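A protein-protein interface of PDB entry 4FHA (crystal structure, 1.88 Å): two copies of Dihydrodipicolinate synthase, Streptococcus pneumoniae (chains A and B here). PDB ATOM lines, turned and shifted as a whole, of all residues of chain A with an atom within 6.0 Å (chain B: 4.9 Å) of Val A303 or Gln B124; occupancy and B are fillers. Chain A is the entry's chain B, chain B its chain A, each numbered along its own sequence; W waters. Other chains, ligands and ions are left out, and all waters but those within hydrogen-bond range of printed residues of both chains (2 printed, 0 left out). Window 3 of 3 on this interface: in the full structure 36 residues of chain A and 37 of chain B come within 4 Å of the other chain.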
ATOM      1  N   TYR A 252      19.056 -19.861  -9.550  1.00  0.00           N
ATOM      2  CA  TYR A 252      19.296 -19.072  -8.350  1.00  0.00           C
ATOM      3  C   TYR A 252      18.870 -19.981  -7.189  1.00  0.00           C
ATOM      4  O   TYR A 252      18.040 -20.869  -7.395  1.00  0.00           O
ATOM      5  CB  TYR A 252      18.492 -17.762  -8.378  1.00  0.00           C
ATOM      6  CG  TYR A 252      19.079 -16.665  -7.510  1.00  0.00           C
ATOM      7  CD1 TYR A 252      20.279 -16.040  -7.863  1.00  0.00           C
ATOM      8  CD2 TYR A 252      18.446 -16.256  -6.332  1.00  0.00           C
ATOM      9  CE1 TYR A 252      20.830 -15.047  -7.070  1.00  0.00           C
ATOM     10  CE2 TYR A 252      18.990 -15.258  -5.532  1.00  0.00           C
ATOM     11  CZ  TYR A 252      20.182 -14.657  -5.910  1.00  0.00           C
ATOM     12  OH  TYR A 252      20.739 -13.672  -5.131  1.00  0.00           O
ATOM     13  N   LEU A 274      15.418 -14.900   5.019  1.00  0.00           N
ATOM     14  CA  LEU A 274      16.880 -14.858   5.111  1.00  0.00           C
ATOM     15  C   LEU A 274      17.407 -16.097   5.849  1.00  0.00           C
ATOM     16  O   LEU A 274      16.771 -16.558   6.794  1.00  0.00           O
ATOM     17  CB  LEU A 274      17.334 -13.574   5.809  1.00  0.00           C
ATOM     18  CG  LEU A 274      17.313 -12.286   4.980  1.00  0.00           C
ATOM     19  CD1 LEU A 274      17.629 -11.086   5.858  1.00  0.00           C
ATOM     20  CD2 LEU A 274      18.285 -12.375   3.810  1.00  0.00           C
ATOM     21  N   VAL A 277      17.505 -15.008  -0.380  1.00  0.00           N
ATOM     22  CA  VAL A 277      16.931 -13.796  -0.966  1.00  0.00           C
ATOM     23  C   VAL A 277      16.172 -14.146  -2.240  1.00  0.00           C
ATOM     24  O   VAL A 277      16.495 -15.137  -2.897  1.00  0.00           O
ATOM     25  CB  VAL A 277      17.996 -12.708  -1.265  1.00  0.00           C
ATOM     26  CG1 VAL A 277      18.547 -12.129   0.031  1.00  0.00           C
ATOM     27  CG2 VAL A 277      19.115 -13.245  -2.155  1.00  0.00           C
ATOM     28  N   PRO A 278      15.145 -13.345  -2.583  1.00  0.00           N
ATOM     29  CA  PRO A 278      14.438 -13.537  -3.846  1.00  0.00           C
ATOM     30  C   PRO A 278      15.380 -13.419  -5.039  1.00  0.00           C
ATOM     31  O   PRO A 278      16.435 -12.777  -4.940  1.00  0.00           O
ATOM     32  CB  PRO A 278      13.433 -12.383  -3.863  1.00  0.00           C
ATOM     33  CG  PRO A 278      13.196 -12.073  -2.430  1.00  0.00           C
ATOM     34  CD  PRO A 278      14.520 -12.292  -1.759  1.00  0.00           C
ATOM     35  N   ALA A 279      15.004 -14.052  -6.146  1.00  0.00           N
ATOM     36  CA  ALA A 279      15.745 -13.943  -7.396  1.00  0.00           C
ATOM     37  C   ALA A 279      15.751 -12.492  -7.885  1.00  0.00           C
ATOM     38  O   ALA A 279      14.739 -11.797  -7.765  1.00  0.00           O
ATOM     39  CB  ALA A 279      15.144 -14.861  -8.448  1.00  0.00           C
ATOM     40  N   PRO A 280      16.901 -12.023  -8.414  1.00  0.00           N
ATOM     41  CA  PRO A 280      16.979 -10.671  -8.982  1.00  0.00           C
ATOM     42  C   PRO A 280      16.070 -10.530 -10.199  1.00  0.00           C
ATOM     43  O   PRO A 280      15.869 -11.500 -10.930  1.00  0.00           O
ATOM     44  CB  PRO A 280      18.449 -10.546  -9.397  1.00  0.00           C
ATOM     45  CG  PRO A 280      19.169 -11.567  -8.582  1.00  0.00           C
ATOM     46  CD  PRO A 280      18.205 -12.707  -8.462  1.00  0.00           C
ATOM     47  N   GLU A 281      15.535  -9.327 -10.404  1.00  0.00           N
ATOM     48  CA  GLU A 281      14.580  -9.046 -11.487  1.00  0.00           C
ATOM     49  C   GLU A 281      15.014  -9.538 -12.869  1.00  0.00           C
ATOM     50  O   GLU A 281      14.186 -10.015 -13.651  1.00  0.00           O
ATOM     51  CB  GLU A 281      14.261  -7.548 -11.539  1.00  0.00           C
ATOM     52  CG  GLU A 281      13.314  -7.079 -10.446  1.00  0.00           C
ATOM     53  CD  GLU A 281      11.885  -7.546 -10.666  1.00  0.00           C
ATOM     54  OE1 GLU A 281      11.352  -7.335 -11.775  1.00  0.00           O
ATOM     55  OE2 GLU A 281      11.293  -8.120  -9.728  1.00  0.00           O
ATOM     56  N   THR A 302      18.086  -4.235  -6.403  1.00  0.00           N
ATOM     57  CA  THR A 302      18.287  -4.928  -5.133  1.00  0.00           C
ATOM     58  C   THR A 302      17.053  -5.747  -4.733  1.00  0.00           C
ATOM     59  O   THR A 302      15.918  -5.393  -5.070  1.00  0.00           O
ATOM     60  CB  THR A 302      18.721  -3.955  -4.001  1.00  0.00           C
ATOM     61  OG1 THR A 302      19.065  -4.694  -2.822  1.00  0.00           O
ATOM     62  CG2 THR A 302      17.625  -2.938  -3.664  1.00  0.00           C
ATOM     63  N   VAL A 303      17.296  -6.852  -4.032  1.00  0.00           N
ATOM     64  CA  VAL A 303      16.236  -7.737  -3.538  1.00  0.00           C
ATOM     65  C   VAL A 303      16.287  -7.817  -2.013  1.00  0.00           C
ATOM     66  O   VAL A 303      17.316  -7.510  -1.407  1.00  0.00           O
ATOM     67  CB  VAL A 303      16.336  -9.158  -4.144  1.00  0.00           C
ATOM     68  CG1 VAL A 303      15.859  -9.157  -5.590  1.00  0.00           C
ATOM     69  CG2 VAL A 303      17.756  -9.703  -4.037  1.00  0.00           C
ATOM     70  N   THR A 304      15.182  -8.227  -1.396  1.00  0.00           N
ATOM     71  CA  THR A 304      15.101  -8.267   0.064  1.00  0.00           C
ATOM     72  C   THR A 304      14.574  -9.608   0.574  1.00  0.00           C
ATOM     73  O   THR A 304      13.439  -9.992   0.282  1.00  0.00           O
ATOM     74  CB  THR A 304      14.222  -7.120   0.616  1.00  0.00           C
ATOM     75  OG1 THR A 304      14.493  -5.909  -0.104  1.00  0.00           O
ATOM     76  CG2 THR A 304      14.490  -6.895   2.100  1.00  0.00           C
ATOM     77  N   GLY A 305      15.417 -10.318   1.321  1.00  0.00           N
ATOM     78  CA  GLY A 305      14.989 -11.497   2.065  1.00  0.00           C
ATOM     79  C   GLY A 305      14.349 -11.041   3.363  1.00  0.00           C
ATOM     80  O   GLY A 305      14.712  -9.994   3.904  1.00  0.00           O
ATOM     81  N   VAL A 306      13.400 -11.824   3.866  1.00  0.00           N
ATOM     82  CA  VAL A 306      12.612 -11.416   5.032  1.00  0.00           C
ATOM     83  C   VAL A 306      12.982 -12.179   6.305  1.00  0.00           C
ATOM     84  O   VAL A 306      13.760 -13.129   6.267  1.00  0.00           O
ATOM     85  CB  VAL A 306      11.091 -11.497   4.754  1.00  0.00           C
ATOM     86  CG1 VAL A 306      10.696 -10.495   3.678  1.00  0.00           C
ATOM     87  CG2 VAL A 306      10.671 -12.909   4.357  1.00  0.00           C
ATOM     88  N   THR B  88      18.759 -16.737   9.847  1.00  0.00           N
ATOM     89  CA  THR B  88      19.148 -15.362  10.161  1.00  0.00           C
ATOM     90  C   THR B  88      18.444 -14.818  11.410  1.00  0.00           C
ATOM     91  O   THR B  88      19.094 -14.236  12.275  1.00  0.00           O
ATOM     92  CB  THR B  88      18.958 -14.424   8.951  1.00  0.00           C
ATOM     93  OG1 THR B  88      19.577 -15.007   7.800  1.00  0.00           O
ATOM     94  CG2 THR B  88      19.583 -13.055   9.206  1.00  0.00           C
ATOM     95  N   GLU B 120      24.399 -12.563  -2.339  1.00  0.00           N
ATOM     96  CA  GLU B 120      23.509 -11.533  -1.801  1.00  0.00           C
ATOM     97  C   GLU B 120      22.766 -12.014  -0.552  1.00  0.00           C
ATOM     98  O   GLU B 120      22.519 -11.234   0.365  1.00  0.00           O
ATOM     99  CB  GLU B 120      22.520 -11.053  -2.872  1.00  0.00           C
ATOM    100  CG  GLU B 120      21.622  -9.893  -2.447  1.00  0.00           C
ATOM    101  CD  GLU B 120      22.384  -8.662  -1.974  1.00  0.00           C
ATOM    102  OE1 GLU B 120      23.530  -8.422  -2.427  1.00  0.00           O
ATOM    103  OE2 GLU B 120      21.827  -7.918  -1.144  1.00  0.00           O
ATOM    104  N   GLY B 121      22.413 -13.297  -0.532  1.00  0.00           N
ATOM    105  CA  GLY B 121      21.822 -13.910   0.652  1.00  0.00           C
ATOM    106  C   GLY B 121      22.775 -13.845   1.828  1.00  0.00           C
ATOM    107  O   GLY B 121      22.422 -13.345   2.898  1.00  0.00           O
ATOM    108  N   MET B 122      23.999 -14.328   1.614  1.00  0.00           N
ATOM    109  CA  MET B 122      25.056 -14.274   2.622  1.00  0.00           C
ATOM    110  C   MET B 122      25.281 -12.855   3.128  1.00  0.00           C
ATOM    111  O   MET B 122      25.375 -12.634   4.333  1.00  0.00           O
ATOM    112  CB  MET B 122      26.372 -14.820   2.060  1.00  0.00           C
ATOM    113  CG  MET B 122      26.309 -16.256   1.576  1.00  0.00           C
ATOM    114  SD  MET B 122      27.882 -16.761   0.861  1.00  0.00           S
ATOM    115  CE  MET B 122      27.421 -18.295   0.071  1.00  0.00           C
ATOM    116  N   TYR B 123      25.368 -11.899   2.201  1.00  0.00           N
ATOM    117  CA  TYR B 123      25.610 -10.501   2.563  1.00  0.00           C
ATOM    118  C   TYR B 123      24.551  -9.976   3.530  1.00  0.00           C
ATOM    119  O   TYR B 123      24.884  -9.431   4.583  1.00  0.00           O
ATOM    120  CB  TYR B 123      25.692  -9.596   1.326  1.00  0.00           C
ATOM    121  CG  TYR B 123      25.938  -8.145   1.688  1.00  0.00           C
ATOM    122  CD1 TYR B 123      27.229  -7.678   1.939  1.00  0.00           C
ATOM    123  CD2 TYR B 123      24.876  -7.246   1.804  1.00  0.00           C
ATOM    124  CE1 TYR B 123      27.456  -6.356   2.292  1.00  0.00           C
ATOM    125  CE2 TYR B 123      25.094  -5.922   2.153  1.00  0.00           C
ATOM    126  CZ  TYR B 123      26.386  -5.485   2.394  1.00  0.00           C
ATOM    127  OH  TYR B 123      26.608  -4.173   2.740  1.00  0.00           O
ATOM    128  N   GLN B 124      23.281 -10.146   3.169  1.00  0.00           N
ATOM    129  CA  GLN B 124      22.172  -9.695   4.011  1.00  0.00           C
ATOM    130  C   GLN B 124      22.114 -10.463   5.333  1.00  0.00           C
ATOM    131  O   GLN B 124      21.799  -9.890   6.373  1.00  0.00           O
ATOM    132  CB  GLN B 124      20.841  -9.784   3.256  1.00  0.00           C
ATOM    133  CG  GLN B 124      20.742  -8.816   2.084  1.00  0.00           C
ATOM    134  CD  GLN B 124      19.393  -8.841   1.385  1.00  0.00           C
ATOM    135  OE1 GLN B 124      18.357  -9.098   2.000  1.00  0.00           O
ATOM    136  NE2 GLN B 124      19.402  -8.558   0.089  1.00  0.00           N
ATOM    137  N   HIS B 125      22.435 -11.755   5.281  1.00  0.00           N
ATOM    138  CA  HIS B 125      22.529 -12.592   6.474  1.00  0.00           C
ATOM    139  C   HIS B 125      23.509 -12.017   7.466  1.00  0.00           C
ATOM    140  O   HIS B 125      23.154 -11.742   8.613  1.00  0.00           O
ATOM    141  CB  HIS B 125      22.913 -14.018   6.080  1.00  0.00           C
ATOM    142  CG  HIS B 125      23.230 -14.919   7.248  1.00  0.00           C
ATOM    143  ND1 HIS B 125      22.273 -15.464   8.022  1.00  0.00           N
ATOM    144  CD2 HIS B 125      24.450 -15.368   7.753  1.00  0.00           C
ATOM    145  CE1 HIS B 125      22.850 -16.227   8.974  1.00  0.00           C
ATOM    146  NE2 HIS B 125      24.181 -16.163   8.809  1.00  0.00           N
ATOM    147  N   PHE B 126      24.747 -11.807   7.024  1.00  0.00           N
ATOM    148  CA  PHE B 126      25.795 -11.293   7.901  1.00  0.00           C
ATOM    149  C   PHE B 126      25.586  -9.836   8.306  1.00  0.00           C
ATOM    150  O   PHE B 126      25.902  -9.456   9.429  1.00  0.00           O
ATOM    151  CB  PHE B 126      27.177 -11.491   7.273  1.00  0.00           C
ATOM    152  CG  PHE B 126      27.598 -12.930   7.195  1.00  0.00           C
ATOM    153  CD1 PHE B 126      27.929 -13.630   8.346  1.00  0.00           C
ATOM    154  CD2 PHE B 126      27.659 -13.584   5.971  1.00  0.00           C
ATOM    155  CE1 PHE B 126      28.307 -14.962   8.280  1.00  0.00           C
ATOM    156  CE2 PHE B 126      28.042 -14.914   5.897  1.00  0.00           C
ATOM    157  CZ  PHE B 126      28.368 -15.601   7.054  1.00  0.00           C
ATOM    158  N   LYS B 127      25.039  -9.035   7.395  1.00  0.00           N
ATOM    159  CA  LYS B 127      24.743  -7.635   7.699  1.00  0.00           C
ATOM    160  C   LYS B 127      23.714  -7.534   8.830  1.00  0.00           C
ATOM    161  O   LYS B 127      23.878  -6.733   9.747  1.00  0.00           O
ATOM    162  CB  LYS B 127      24.260  -6.898   6.448  1.00  0.00           C
ATOM    163  CG  LYS B 127      24.209  -5.386   6.599  1.00  0.00           C
ATOM    164  CD  LYS B 127      23.605  -4.733   5.364  1.00  0.00           C
ATOM    165  CE  LYS B 127      23.300  -3.262   5.617  1.00  0.00           C
ATOM    166  NZ  LYS B 127      22.294  -3.082   6.701  1.00  0.00           N
ATOM    167  N   ALA B 128      22.674  -8.366   8.770  1.00  0.00           N
ATOM    168  CA  ALA B 128      21.635  -8.393   9.804  1.00  0.00           C
ATOM    169  C   ALA B 128      22.190  -8.790  11.172  1.00  0.00           C
ATOM    170  O   ALA B 128      21.806  -8.217  12.188  1.00  0.00           O
ATOM    171  CB  ALA B 128      20.491  -9.312   9.399  1.00  0.00           C
HETATM  172  O   HOH W   1      15.708 -15.767   9.238  1.00  0.00           O
HETATM  173  O   HOH W   2      24.021 -13.011  -5.266  1.00  0.00           O
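OG1 of Thr B88 sits close to O of Leu A274 (3.4 Å). O of Val A303 lies within hydrogen-bond range of NE2 of Gln B124 (2.8 Å). N of Gly A305 lies within hydrogen-bond range of OE1 of Gln B124 (3.3 Å).
The side-chain hydroxyl of Thr B88 is in hydrogen-bond range of a ring nitrogen (ND1) of His B125, at 2.7 Å. OE2 of Glu B120 lies within hydrogen-bond range of NE2 of Gln B124. The backbone NH of Leu A274 lies within hydrogen-bond range of the backbone carbonyl oxygen of Val A306, 2.7 Å away.
OH of Tyr A252 touches CB of Glu B120, at 3.9 Å. CD2 of Leu A274 touches CB of Gln B124 (3.7 Å). Val A277 touches Gly B121 (CG2 to N, 3.7 Å). Gln B124 touches Val A277 (OE1 to CG1, 3.6 Å). CA of Thr A304 touches OE1 of Gln B124 (3.9 Å).
Of the printed residues of chain B, Tyr A252 touches Glu B120 (3.9 Å). Of the printed residues of chain B, Val A277 touches Gly B121 (3.7 Å) and Gln B124 (3.6 Å). Printed residues of chain B within 4 Å of Val A303: Gln B124 (2.8 Å). Printed residues of chain B within 4 Å of Thr A304: Gln B124 (3.9 Å). Gln B124 touches just these residues of chain A: Leu A274 (3.7 Å), Val A277 (3.6 Å), Val A303 (2.8 Å), Thr A304 (3.9 Å) and Gly A305 (3.3 Å). Lys B127 touches none of the printed residues of chain A. The nearest printed residue of chain A that does not touch Glu B120 is Val A277 (4.1 Å).
No position is printed for both chains. Of the 8 pairs that touch across the chains among the printed residues, none has its exchanged pair printed and touching as well.
Water W1 lies within hydrogen-bond range of O of Leu A274 and N of Thr B88. Water W2 bridges N of Glu B120 and OH of Tyr A252.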
